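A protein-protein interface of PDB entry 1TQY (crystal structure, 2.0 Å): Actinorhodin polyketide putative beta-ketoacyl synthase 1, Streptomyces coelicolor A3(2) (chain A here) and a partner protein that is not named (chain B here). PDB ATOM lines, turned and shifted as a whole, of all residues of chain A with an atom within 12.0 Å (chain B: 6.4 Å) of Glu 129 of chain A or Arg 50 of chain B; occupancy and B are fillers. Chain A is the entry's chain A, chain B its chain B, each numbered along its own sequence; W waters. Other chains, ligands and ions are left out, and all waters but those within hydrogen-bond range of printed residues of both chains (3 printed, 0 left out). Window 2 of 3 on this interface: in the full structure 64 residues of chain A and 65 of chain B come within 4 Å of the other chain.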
ATOM      1  N   GLU A 117      13.688  29.917 -19.262  1.00  0.00           N
ATOM      2  CA  GLU A 117      14.672  28.966 -19.738  1.00  0.00           C
ATOM      3  C   GLU A 117      14.619  27.654 -18.968  1.00  0.00           C
ATOM      4  O   GLU A 117      14.838  26.589 -19.546  1.00  0.00           O
ATOM      5  CB  GLU A 117      16.080  29.554 -19.644  1.00  0.00           C
ATOM      6  CG  GLU A 117      16.271  30.836 -20.441  1.00  0.00           C
ATOM      7  CD  GLU A 117      15.816  30.697 -21.884  1.00  0.00           C
ATOM      8  OE1 GLU A 117      16.127  29.668 -22.532  1.00  0.00           O
ATOM      9  OE2 GLU A 117      15.152  31.624 -22.388  1.00  0.00           O
ATOM     10  N   TYR A 118      14.332  27.714 -17.671  1.00  0.00           N
ATOM     11  CA  TYR A 118      14.284  26.487 -16.883  1.00  0.00           C
ATOM     12  C   TYR A 118      13.311  25.463 -17.466  1.00  0.00           C
ATOM     13  O   TYR A 118      13.624  24.280 -17.516  1.00  0.00           O
ATOM     14  CB  TYR A 118      13.908  26.765 -15.419  1.00  0.00           C
ATOM     15  CG  TYR A 118      13.758  25.473 -14.634  1.00  0.00           C
ATOM     16  CD1 TYR A 118      14.881  24.725 -14.259  1.00  0.00           C
ATOM     17  CD2 TYR A 118      12.491  24.929 -14.388  1.00  0.00           C
ATOM     18  CE1 TYR A 118      14.746  23.462 -13.676  1.00  0.00           C
ATOM     19  CE2 TYR A 118      12.343  23.670 -13.808  1.00  0.00           C
ATOM     20  CZ  TYR A 118      13.472  22.941 -13.462  1.00  0.00           C
ATOM     21  OH  TYR A 118      13.317  21.674 -12.956  1.00  0.00           O
ATOM     22  N   LEU A 119      12.140  25.915 -17.915  1.00  0.00           N
ATOM     23  CA  LEU A 119      11.158  25.003 -18.484  1.00  0.00           C
ATOM     24  C   LEU A 119      11.673  24.310 -19.750  1.00  0.00           C
ATOM     25  O   LEU A 119      11.397  23.132 -19.977  1.00  0.00           O
ATOM     26  CB  LEU A 119       9.846  25.736 -18.786  1.00  0.00           C
ATOM     27  CG  LEU A 119       8.761  25.767 -17.697  1.00  0.00           C
ATOM     28  CD1 LEU A 119       9.337  26.099 -16.343  1.00  0.00           C
ATOM     29  CD2 LEU A 119       7.694  26.764 -18.099  1.00  0.00           C
ATOM     30  N   LEU A 120      12.429  25.018 -20.577  1.00  0.00           N
ATOM     31  CA  LEU A 120      12.928  24.376 -21.782  1.00  0.00           C
ATOM     32  C   LEU A 120      14.047  23.385 -21.468  1.00  0.00           C
ATOM     33  O   LEU A 120      14.105  22.310 -22.053  1.00  0.00           O
ATOM     34  CB  LEU A 120      13.431  25.411 -22.788  1.00  0.00           C
ATOM     35  CG  LEU A 120      12.434  26.386 -23.409  1.00  0.00           C
ATOM     36  CD1 LEU A 120      13.189  27.158 -24.481  1.00  0.00           C
ATOM     37  CD2 LEU A 120      11.216  25.669 -24.011  1.00  0.00           C
ATOM     38  N   LEU A 121      14.920  23.737 -20.536  1.00  0.00           N
ATOM     39  CA  LEU A 121      16.040  22.868 -20.184  1.00  0.00           C
ATOM     40  C   LEU A 121      15.696  21.592 -19.426  1.00  0.00           C
ATOM     41  O   LEU A 121      16.286  20.541 -19.658  1.00  0.00           O
ATOM     42  CB  LEU A 121      17.048  23.658 -19.368  1.00  0.00           C
ATOM     43  CG  LEU A 121      17.872  24.593 -20.240  1.00  0.00           C
ATOM     44  CD1 LEU A 121      18.334  25.800 -19.436  1.00  0.00           C
ATOM     45  CD2 LEU A 121      19.051  23.821 -20.819  1.00  0.00           C
ATOM     46  N   SER A 122      14.738  21.704 -18.521  1.00  0.00           N
ATOM     47  CA  SER A 122      14.337  20.599 -17.684  1.00  0.00           C
ATOM     48  C   SER A 122      13.135  19.814 -18.205  1.00  0.00           C
ATOM     49  O   SER A 122      12.747  18.801 -17.614  1.00  0.00           O
ATOM     50  CB  SER A 122      14.004  21.137 -16.284  1.00  0.00           C
ATOM     51  OG  SER A 122      12.823  21.940 -16.301  1.00  0.00           O
ATOM     52  N   ASP A 123      12.557  20.282 -19.308  1.00  0.00           N
ATOM     53  CA  ASP A 123      11.354  19.687 -19.893  1.00  0.00           C
ATOM     54  C   ASP A 123      10.252  19.874 -18.850  1.00  0.00           C
ATOM     55  O   ASP A 123       9.600  18.921 -18.422  1.00  0.00           O
ATOM     56  CB  ASP A 123      11.533  18.193 -20.192  1.00  0.00           C
ATOM     57  CG  ASP A 123      10.402  17.624 -21.055  1.00  0.00           C
ATOM     58  OD1 ASP A 123      10.388  16.394 -21.308  1.00  0.00           O
ATOM     59  OD2 ASP A 123       9.527  18.397 -21.495  1.00  0.00           O
ATOM     60  N   SER A 124      10.092  21.116 -18.413  1.00  0.00           N
ATOM     61  CA  SER A 124       9.083  21.480 -17.428  1.00  0.00           C
ATOM     62  C   SER A 124       9.209  20.760 -16.086  1.00  0.00           C
ATOM     63  O   SER A 124       8.224  20.240 -15.564  1.00  0.00           O
ATOM     64  CB  SER A 124       7.682  21.266 -18.015  1.00  0.00           C
ATOM     65  OG  SER A 124       7.480  22.114 -19.134  1.00  0.00           O
ATOM     66  N   GLY A 125      10.425  20.733 -15.543  1.00  0.00           N
ATOM     67  CA  GLY A 125      10.656  20.121 -14.249  1.00  0.00           C
ATOM     68  C   GLY A 125      10.870  18.620 -14.200  1.00  0.00           C
ATOM     69  O   GLY A 125      11.063  18.064 -13.120  1.00  0.00           O
ATOM     70  N   ARG A 126      10.848  17.956 -15.350  1.00  0.00           N
ATOM     71  CA  ARG A 126      11.026  16.510 -15.395  1.00  0.00           C
ATOM     72  C   ARG A 126      12.452  16.042 -15.134  1.00  0.00           C
ATOM     73  O   ARG A 126      12.660  15.033 -14.460  1.00  0.00           O
ATOM     74  CB  ARG A 126      10.562  15.959 -16.749  1.00  0.00           C
ATOM     75  CG  ARG A 126       9.051  15.960 -16.923  1.00  0.00           C
ATOM     76  CD  ARG A 126       8.632  15.362 -18.252  1.00  0.00           C
ATOM     77  NE  ARG A 126       7.187  15.114 -18.318  1.00  0.00           N
ATOM     78  CZ  ARG A 126       6.259  16.068 -18.351  1.00  0.00           C
ATOM     79  NH1 ARG A 126       6.618  17.345 -18.326  1.00  0.00           N
ATOM     80  NH2 ARG A 126       4.973  15.744 -18.398  1.00  0.00           N
ATOM     81  N   ASP A 127      13.429  16.785 -15.643  1.00  0.00           N
ATOM     82  CA  ASP A 127      14.821  16.392 -15.504  1.00  0.00           C
ATOM     83  C   ASP A 127      15.751  17.329 -14.739  1.00  0.00           C
ATOM     84  O   ASP A 127      15.782  18.538 -14.989  1.00  0.00           O
ATOM     85  CB  ASP A 127      15.410  16.127 -16.900  1.00  0.00           C
ATOM     86  CG  ASP A 127      14.558  15.175 -17.724  1.00  0.00           C
ATOM     87  OD1 ASP A 127      14.227  14.090 -17.205  1.00  0.00           O
ATOM     88  OD2 ASP A 127      14.212  15.515 -18.884  1.00  0.00           O
ATOM     89  N   TRP A 128      16.514  16.751 -13.810  1.00  0.00           N
ATOM     90  CA  TRP A 128      17.494  17.489 -13.006  1.00  0.00           C
ATOM     91  C   TRP A 128      18.707  17.713 -13.900  1.00  0.00           C
ATOM     92  O   TRP A 128      19.312  18.780 -13.885  1.00  0.00           O
ATOM     93  CB  TRP A 128      17.904  16.664 -11.778  1.00  0.00           C
ATOM     94  CG  TRP A 128      19.016  17.259 -10.961  1.00  0.00           C
ATOM     95  CD1 TRP A 128      20.271  16.753 -10.798  1.00  0.00           C
ATOM     96  CD2 TRP A 128      18.963  18.457 -10.176  1.00  0.00           C
ATOM     97  NE1 TRP A 128      21.004  17.554  -9.961  1.00  0.00           N
ATOM     98  CE2 TRP A 128      20.228  18.612  -9.561  1.00  0.00           C
ATOM     99  CE3 TRP A 128      17.969  19.416  -9.933  1.00  0.00           C
ATOM    100  CZ2 TRP A 128      20.528  19.695  -8.711  1.00  0.00           C
ATOM    101  CZ3 TRP A 128      18.266  20.490  -9.091  1.00  0.00           C
ATOM    102  CH2 TRP A 128      19.534  20.621  -8.490  1.00  0.00           C
ATOM    103  N   GLU A 129      19.071  16.681 -14.658  1.00  0.00           N
ATOM    104  CA  GLU A 129      20.191  16.783 -15.587  1.00  0.00           C
ATOM    105  C   GLU A 129      19.608  17.355 -16.872  1.00  0.00           C
ATOM    106  O   GLU A 129      19.225  16.622 -17.788  1.00  0.00           O
ATOM    107  CB  GLU A 129      20.826  15.407 -15.819  1.00  0.00           C
ATOM    108  CG  GLU A 129      22.114  15.215 -15.034  1.00  0.00           C
ATOM    109  CD  GLU A 129      22.468  13.762 -14.786  1.00  0.00           C
ATOM    110  OE1 GLU A 129      22.475  12.966 -15.754  1.00  0.00           O
ATOM    111  OE2 GLU A 129      22.756  13.412 -13.617  1.00  0.00           O
ATOM    112  N   VAL A 130      19.530  18.681 -16.905  1.00  0.00           N
ATOM    113  CA  VAL A 130      18.950  19.407 -18.027  1.00  0.00           C
ATOM    114  C   VAL A 130      19.611  19.096 -19.353  1.00  0.00           C
ATOM    115  O   VAL A 130      20.768  18.682 -19.398  1.00  0.00           O
ATOM    116  CB  VAL A 130      18.984  20.926 -17.765  1.00  0.00           C
ATOM    117  CG1 VAL A 130      18.058  21.260 -16.601  1.00  0.00           C
ATOM    118  CG2 VAL A 130      20.420  21.377 -17.458  1.00  0.00           C
ATOM    119  N   ASP A 131      18.850  19.291 -20.426  1.00  0.00           N
ATOM    120  CA  ASP A 131      19.304  19.009 -21.782  1.00  0.00           C
ATOM    121  C   ASP A 131      19.906  20.218 -22.502  1.00  0.00           C
ATOM    122  O   ASP A 131      19.192  21.113 -22.952  1.00  0.00           O
ATOM    123  CB  ASP A 131      18.125  18.447 -22.581  1.00  0.00           C
ATOM    124  CG  ASP A 131      18.515  17.996 -23.987  1.00  0.00           C
ATOM    125  OD1 ASP A 131      17.650  17.435 -24.682  1.00  0.00           O
ATOM    126  OD2 ASP A 131      19.671  18.204 -24.392  1.00  0.00           O
ATOM    127  N   ALA A 132      21.228  20.215 -22.621  1.00  0.00           N
ATOM    128  CA  ALA A 132      21.955  21.296 -23.265  1.00  0.00           C
ATOM    129  C   ALA A 132      21.475  21.582 -24.687  1.00  0.00           C
ATOM    130  O   ALA A 132      21.851  22.594 -25.280  1.00  0.00           O
ATOM    131  CB  ALA A 132      23.458  20.979 -23.269  1.00  0.00           C
ATOM    132  N   ALA A 133      20.652  20.697 -25.242  1.00  0.00           N
ATOM    133  CA  ALA A 133      20.133  20.897 -26.591  1.00  0.00           C
ATOM    134  C   ALA A 133      19.201  22.107 -26.614  1.00  0.00           C
ATOM    135  O   ALA A 133      19.005  22.731 -27.654  1.00  0.00           O
ATOM    136  CB  ALA A 133      19.377  19.644 -27.055  1.00  0.00           C
ATOM    137  N   TRP A 134      18.630  22.436 -25.457  1.00  0.00           N
ATOM    138  CA  TRP A 134      17.711  23.567 -25.337  1.00  0.00           C
ATOM    139  C   TRP A 134      18.337  24.757 -24.588  1.00  0.00           C
ATOM    140  O   TRP A 134      17.620  25.586 -24.033  1.00  0.00           O
ATOM    141  CB  TRP A 134      16.434  23.131 -24.601  1.00  0.00           C
ATOM    142  CG  TRP A 134      15.694  22.026 -25.281  1.00  0.00           C
ATOM    143  CD1 TRP A 134      15.958  20.683 -25.196  1.00  0.00           C
ATOM    144  CD2 TRP A 134      14.616  22.162 -26.219  1.00  0.00           C
ATOM    145  NE1 TRP A 134      15.116  19.983 -26.023  1.00  0.00           N
ATOM    146  CE2 TRP A 134      14.286  20.865 -26.664  1.00  0.00           C
ATOM    147  CE3 TRP A 134      13.900  23.255 -26.727  1.00  0.00           C
ATOM    148  CZ2 TRP A 134      13.277  20.629 -27.593  1.00  0.00           C
ATOM    149  CZ3 TRP A 134      12.885  23.020 -27.659  1.00  0.00           C
ATOM    150  CH2 TRP A 134      12.586  21.716 -28.081  1.00  0.00           C
ATOM    151  N   LEU A 135      19.667  24.828 -24.590  1.00  0.00           N
ATOM    152  CA  LEU A 135      20.416  25.876 -23.902  1.00  0.00           C
ATOM    153  C   LEU A 135      20.342  27.233 -24.589  1.00  0.00           C
ATOM    154  O   LEU A 135      20.759  27.369 -25.746  1.00  0.00           O
ATOM    155  CB  LEU A 135      21.887  25.465 -23.795  1.00  0.00           C
ATOM    156  CG  LEU A 135      22.768  25.918 -22.642  1.00  0.00           C
ATOM    157  CD1 LEU A 135      24.233  25.762 -23.066  1.00  0.00           C
ATOM    158  CD2 LEU A 135      22.480  27.346 -22.261  1.00  0.00           C
ATOM    159  N   ARG B  45      29.500  16.149  -9.194  1.00  0.00           N
ATOM    160  CA  ARG B  45      28.252  16.614  -8.601  1.00  0.00           C
ATOM    161  C   ARG B  45      27.042  16.035  -9.329  1.00  0.00           C
ATOM    162  O   ARG B  45      25.940  16.005  -8.791  1.00  0.00           O
ATOM    163  CB  ARG B  45      28.198  18.145  -8.636  1.00  0.00           C
ATOM    164  CG  ARG B  45      29.280  18.822  -7.809  1.00  0.00           C
ATOM    165  CD  ARG B  45      29.138  18.463  -6.339  1.00  0.00           C
ATOM    166  NE  ARG B  45      30.386  18.650  -5.610  1.00  0.00           N
ATOM    167  CZ  ARG B  45      30.747  19.774  -5.004  1.00  0.00           C
ATOM    168  NH1 ARG B  45      29.945  20.835  -5.031  1.00  0.00           N
ATOM    169  NH2 ARG B  45      31.914  19.833  -4.375  1.00  0.00           N
ATOM    170  N   PHE B  46      27.267  15.575 -10.557  1.00  0.00           N
ATOM    171  CA  PHE B  46      26.225  14.988 -11.396  1.00  0.00           C
ATOM    172  C   PHE B  46      26.950  14.356 -12.582  1.00  0.00           C
ATOM    173  O   PHE B  46      28.175  14.358 -12.609  1.00  0.00           O
ATOM    174  CB  PHE B  46      25.249  16.074 -11.855  1.00  0.00           C
ATOM    175  CG  PHE B  46      25.913  17.213 -12.565  1.00  0.00           C
ATOM    176  CD1 PHE B  46      26.217  17.115 -13.920  1.00  0.00           C
ATOM    177  CD2 PHE B  46      26.278  18.364 -11.873  1.00  0.00           C
ATOM    178  CE1 PHE B  46      26.878  18.145 -14.582  1.00  0.00           C
ATOM    179  CE2 PHE B  46      26.940  19.405 -12.519  1.00  0.00           C
ATOM    180  CZ  PHE B  46      27.243  19.292 -13.884  1.00  0.00           C
ATOM    181  N   ASP B  47      26.213  13.819 -13.550  1.00  0.00           N
ATOM    182  CA  ASP B  47      26.824  13.164 -14.717  1.00  0.00           C
ATOM    183  C   ASP B  47      27.220  14.148 -15.825  1.00  0.00           C
ATOM    184  O   ASP B  47      26.416  14.435 -16.707  1.00  0.00           O
ATOM    185  CB  ASP B  47      25.839  12.130 -15.291  1.00  0.00           C
ATOM    186  CG  ASP B  47      26.497  11.152 -16.258  1.00  0.00           C
ATOM    187  OD1 ASP B  47      27.608  11.443 -16.752  1.00  0.00           O
ATOM    188  OD2 ASP B  47      25.891  10.096 -16.533  1.00  0.00           O
ATOM    189  N   VAL B  48      28.456  14.645 -15.796  1.00  0.00           N
ATOM    190  CA  VAL B  48      28.926  15.599 -16.809  1.00  0.00           C
ATOM    191  C   VAL B  48      29.293  15.008 -18.159  1.00  0.00           C
ATOM    192  O   VAL B  48      29.518  15.750 -19.117  1.00  0.00           O
ATOM    193  CB  VAL B  48      30.184  16.384 -16.366  1.00  0.00           C
ATOM    194  CG1 VAL B  48      29.796  17.586 -15.568  1.00  0.00           C
ATOM    195  CG2 VAL B  48      31.126  15.474 -15.598  1.00  0.00           C
ATOM    196  N   SER B  49      29.379  13.687 -18.242  1.00  0.00           N
ATOM    197  CA  SER B  49      29.743  13.035 -19.494  1.00  0.00           C
ATOM    198  C   SER B  49      28.760  13.379 -20.595  1.00  0.00           C
ATOM    199  O   SER B  49      29.036  13.160 -21.769  1.00  0.00           O
ATOM    200  CB  SER B  49      29.754  11.519 -19.322  1.00  0.00           C
ATOM    201  OG  SER B  49      28.432  11.026 -19.159  1.00  0.00           O
ATOM    202  N   ARG B  50      27.602  13.901 -20.226  1.00  0.00           N
ATOM    203  CA  ARG B  50      26.626  14.231 -21.244  1.00  0.00           C
ATOM    204  C   ARG B  50      26.692  15.688 -21.686  1.00  0.00           C
ATOM    205  O   ARG B  50      25.878  16.140 -22.484  1.00  0.00           O
ATOM    206  CB  ARG B  50      25.228  13.875 -20.753  1.00  0.00           C
ATOM    207  CG  ARG B  50      24.863  14.479 -19.416  1.00  0.00           C
ATOM    208  CD  ARG B  50      23.747  13.699 -18.779  1.00  0.00           C
ATOM    209  NE  ARG B  50      22.543  13.670 -19.619  1.00  0.00           N
ATOM    210  CZ  ARG B  50      21.369  13.196 -19.211  1.00  0.00           C
ATOM    211  NH1 ARG B  50      20.338  13.181 -20.028  1.00  0.00           N
ATOM    212  NH2 ARG B  50      21.227  12.734 -17.980  1.00  0.00           N
ATOM    213  N   TYR B  51      27.669  16.420 -21.164  1.00  0.00           N
ATOM    214  CA  TYR B  51      27.856  17.825 -21.522  1.00  0.00           C
ATOM    215  C   TYR B  51      29.245  18.036 -22.125  1.00  0.00           C
ATOM    216  O   TYR B  51      30.169  17.267 -21.855  1.00  0.00           O
ATOM    217  CB  TYR B  51      27.705  18.702 -20.281  1.00  0.00           C
ATOM    218  CG  TYR B  51      26.363  18.571 -19.619  1.00  0.00           C
ATOM    219  CD1 TYR B  51      25.213  19.065 -20.224  1.00  0.00           C
ATOM    220  CD2 TYR B  51      26.241  17.936 -18.386  1.00  0.00           C
ATOM    221  CE1 TYR B  51      23.972  18.927 -19.609  1.00  0.00           C
ATOM    222  CE2 TYR B  51      25.008  17.794 -17.769  1.00  0.00           C
ATOM    223  CZ  TYR B  51      23.880  18.290 -18.383  1.00  0.00           C
ATOM    224  OH  TYR B  51      22.666  18.162 -17.763  1.00  0.00           O
ATOM    225  N   PRO B  52      29.410  19.090 -22.938  1.00  0.00           N
ATOM    226  CA  PRO B  52      30.680  19.432 -23.595  1.00  0.00           C
ATOM    227  C   PRO B  52      31.835  19.673 -22.624  1.00  0.00           C
ATOM    228  O   PRO B  52      32.933  19.166 -22.818  1.00  0.00           O
ATOM    229  CB  PRO B  52      30.347  20.706 -24.369  1.00  0.00           C
ATOM    230  CG  PRO B  52      28.886  20.598 -24.615  1.00  0.00           C
ATOM    231  CD  PRO B  52      28.348  20.029 -23.332  1.00  0.00           C
ATOM    232  N   THR B  54      33.550  19.274 -18.919  1.00  0.00           N
ATOM    233  CA  THR B  54      33.489  18.275 -17.859  1.00  0.00           C
ATOM    234  C   THR B  54      34.428  18.513 -16.691  1.00  0.00           C
ATOM    235  O   THR B  54      34.390  17.781 -15.701  1.00  0.00           O
ATOM    236  CB  THR B  54      33.830  16.887 -18.412  1.00  0.00           C
ATOM    237  OG1 THR B  54      35.176  16.906 -18.905  1.00  0.00           O
ATOM    238  CG2 THR B  54      32.892  16.515 -19.539  1.00  0.00           C
ATOM    239  N   HIS B 121      17.675  25.953  -8.082  1.00  0.00           N
ATOM    240  CA  HIS B 121      17.361  24.979  -9.130  1.00  0.00           C
ATOM    241  C   HIS B 121      16.423  23.914  -8.552  1.00  0.00           C
ATOM    242  O   HIS B 121      15.398  23.573  -9.150  1.00  0.00           O
ATOM    243  CB  HIS B 121      18.640  24.322  -9.652  1.00  0.00           C
ATOM    244  CG  HIS B 121      18.419  23.345 -10.771  1.00  0.00           C
ATOM    245  ND1 HIS B 121      19.435  22.563 -11.278  1.00  0.00           N
ATOM    246  CD2 HIS B 121      17.303  23.000 -11.458  1.00  0.00           C
ATOM    247  CE1 HIS B 121      18.954  21.779 -12.227  1.00  0.00           C
ATOM    248  NE2 HIS B 121      17.664  22.023 -12.355  1.00  0.00           N
ATOM    249  N   PRO B 201      23.537  20.775 -12.526  1.00  0.00           N
ATOM    250  CA  PRO B 201      23.360  20.711 -13.980  1.00  0.00           C
ATOM    251  C   PRO B 201      23.002  22.042 -14.662  1.00  0.00           C
ATOM    252  O   PRO B 201      23.584  22.378 -15.688  1.00  0.00           O
ATOM    253  CB  PRO B 201      22.267  19.666 -14.143  1.00  0.00           C
ATOM    254  CG  PRO B 201      22.460  18.772 -12.936  1.00  0.00           C
ATOM    255  CD  PRO B 201      22.704  19.762 -11.843  1.00  0.00           C
HETATM  256  O   HOH W   1      22.809  17.719 -22.688  1.00  0.00           O
HETATM  257  O   HOH W   2      23.549  17.804  -8.853  1.00  0.00           O
HETATM  258  O   HOH W   3      15.548  20.492 -13.038  1.00  0.00           O
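NH2 of Arg 50 of chain B is in salt-bridge range of OE1 of Glu 129 of chain A (2.6 Å). The backbone carbonyl oxygen of Val 130 of chain A sits at hydrogen-bond distance from the side-chain hydroxyl of Tyr 51 of chain B, 2.6 Å away. The side-chain carboxylate (OE2) of Glu 129 of chain A lies within hydrogen-bond range of the backbone NH (N) of Asp 47 of chain B, 3.5 Å away.
O of Tyr 118 of chain A lies within hydrogen-bond range of OG of Ser 122 of chain A (2.8 Å). The side-chain hydroxyl (OG) of Ser 49 of chain B lies within hydrogen-bond range of the side-chain carboxylate (OD1) of Asp 47 of chain B (2.6 Å).
Among the printed residues, pairs that only touch across the chains: Trp 128 of chain A with Pro 201 of chain B (3.1 Å), Trp 128 of chain A with His 121 of chain B (3.2 Å), Glu 129 of chain A with Tyr 51 of chain B (3.3 Å), Tyr 118 of chain A with His 121 of chain B (3.4 Å), Val 130 of chain A with Pro 201 of chain B (3.8 Å) and Glu 129 of chain A with Pro 201 of chain B (3.8 Å).
Glu 117 of chain A touches none of the printed residues of chain B. Of the printed residues of chain B, Trp 128 of chain A touches His 121 and Pro 201. Glu 129 of chain A touches just these residues of chain B: Asp 47 (3.5 Å), Arg 50 (2.6 Å), Tyr 51 (3.3 Å) and Pro 201 (3.8 Å). No residue of chain A comes within 4 Å of Phe 46 of chain B. Asp 47 of chain B touches just one residue of chain A: Glu 129 (3.5 Å). No residue of chain A comes within 4 Å of Val 48 of chain B. Arg 50 of chain B touches just one residue of chain A: Glu 129. Of the printed residues of chain A, Tyr 51 of chain B touches Glu 129 and Val 130. No residue of chain A comes within 4 Å of Pro 52 of chain B. Of the printed residues of chain A, His 121 of chain B touches Tyr 118 and Trp 128. The nearest residue of chain A that does not touch Arg 50 of chain B is Val 130 of chain A (5.3 Å). The nearest printed residue of chain B that does not touch Val 130 of chain A is His 121 of chain B (4.3 Å).
Hydrophobic or aromatic side chains of chain A within 4 Å of the printed part of chain B: Tyr 118, Trp 128 and Val 130. Among the printed residues, Asp or Glu carboxylates within 4 Å of a Lys or Arg side-chain nitrogen of the other chain: Glu 129 of chain A with Arg 50 of chain B (2.6 Å).
Water W3 lies within hydrogen-bond range of OH of Tyr 118 of chain A (2.5 Å), NE2 of His 121 of chain B (2.7 Å) and O of Asp 127 of chain A (2.8 Å). Water W2 bridges NE1 of Trp 128 of chain A and O of Arg 45 of chain B. Water W1 bridges the backbone NH (N) of Ala 132 of chain A (3.0 Å) and the backbone carbonyl oxygen (O) of Arg 50 of chain B (3.5 Å).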
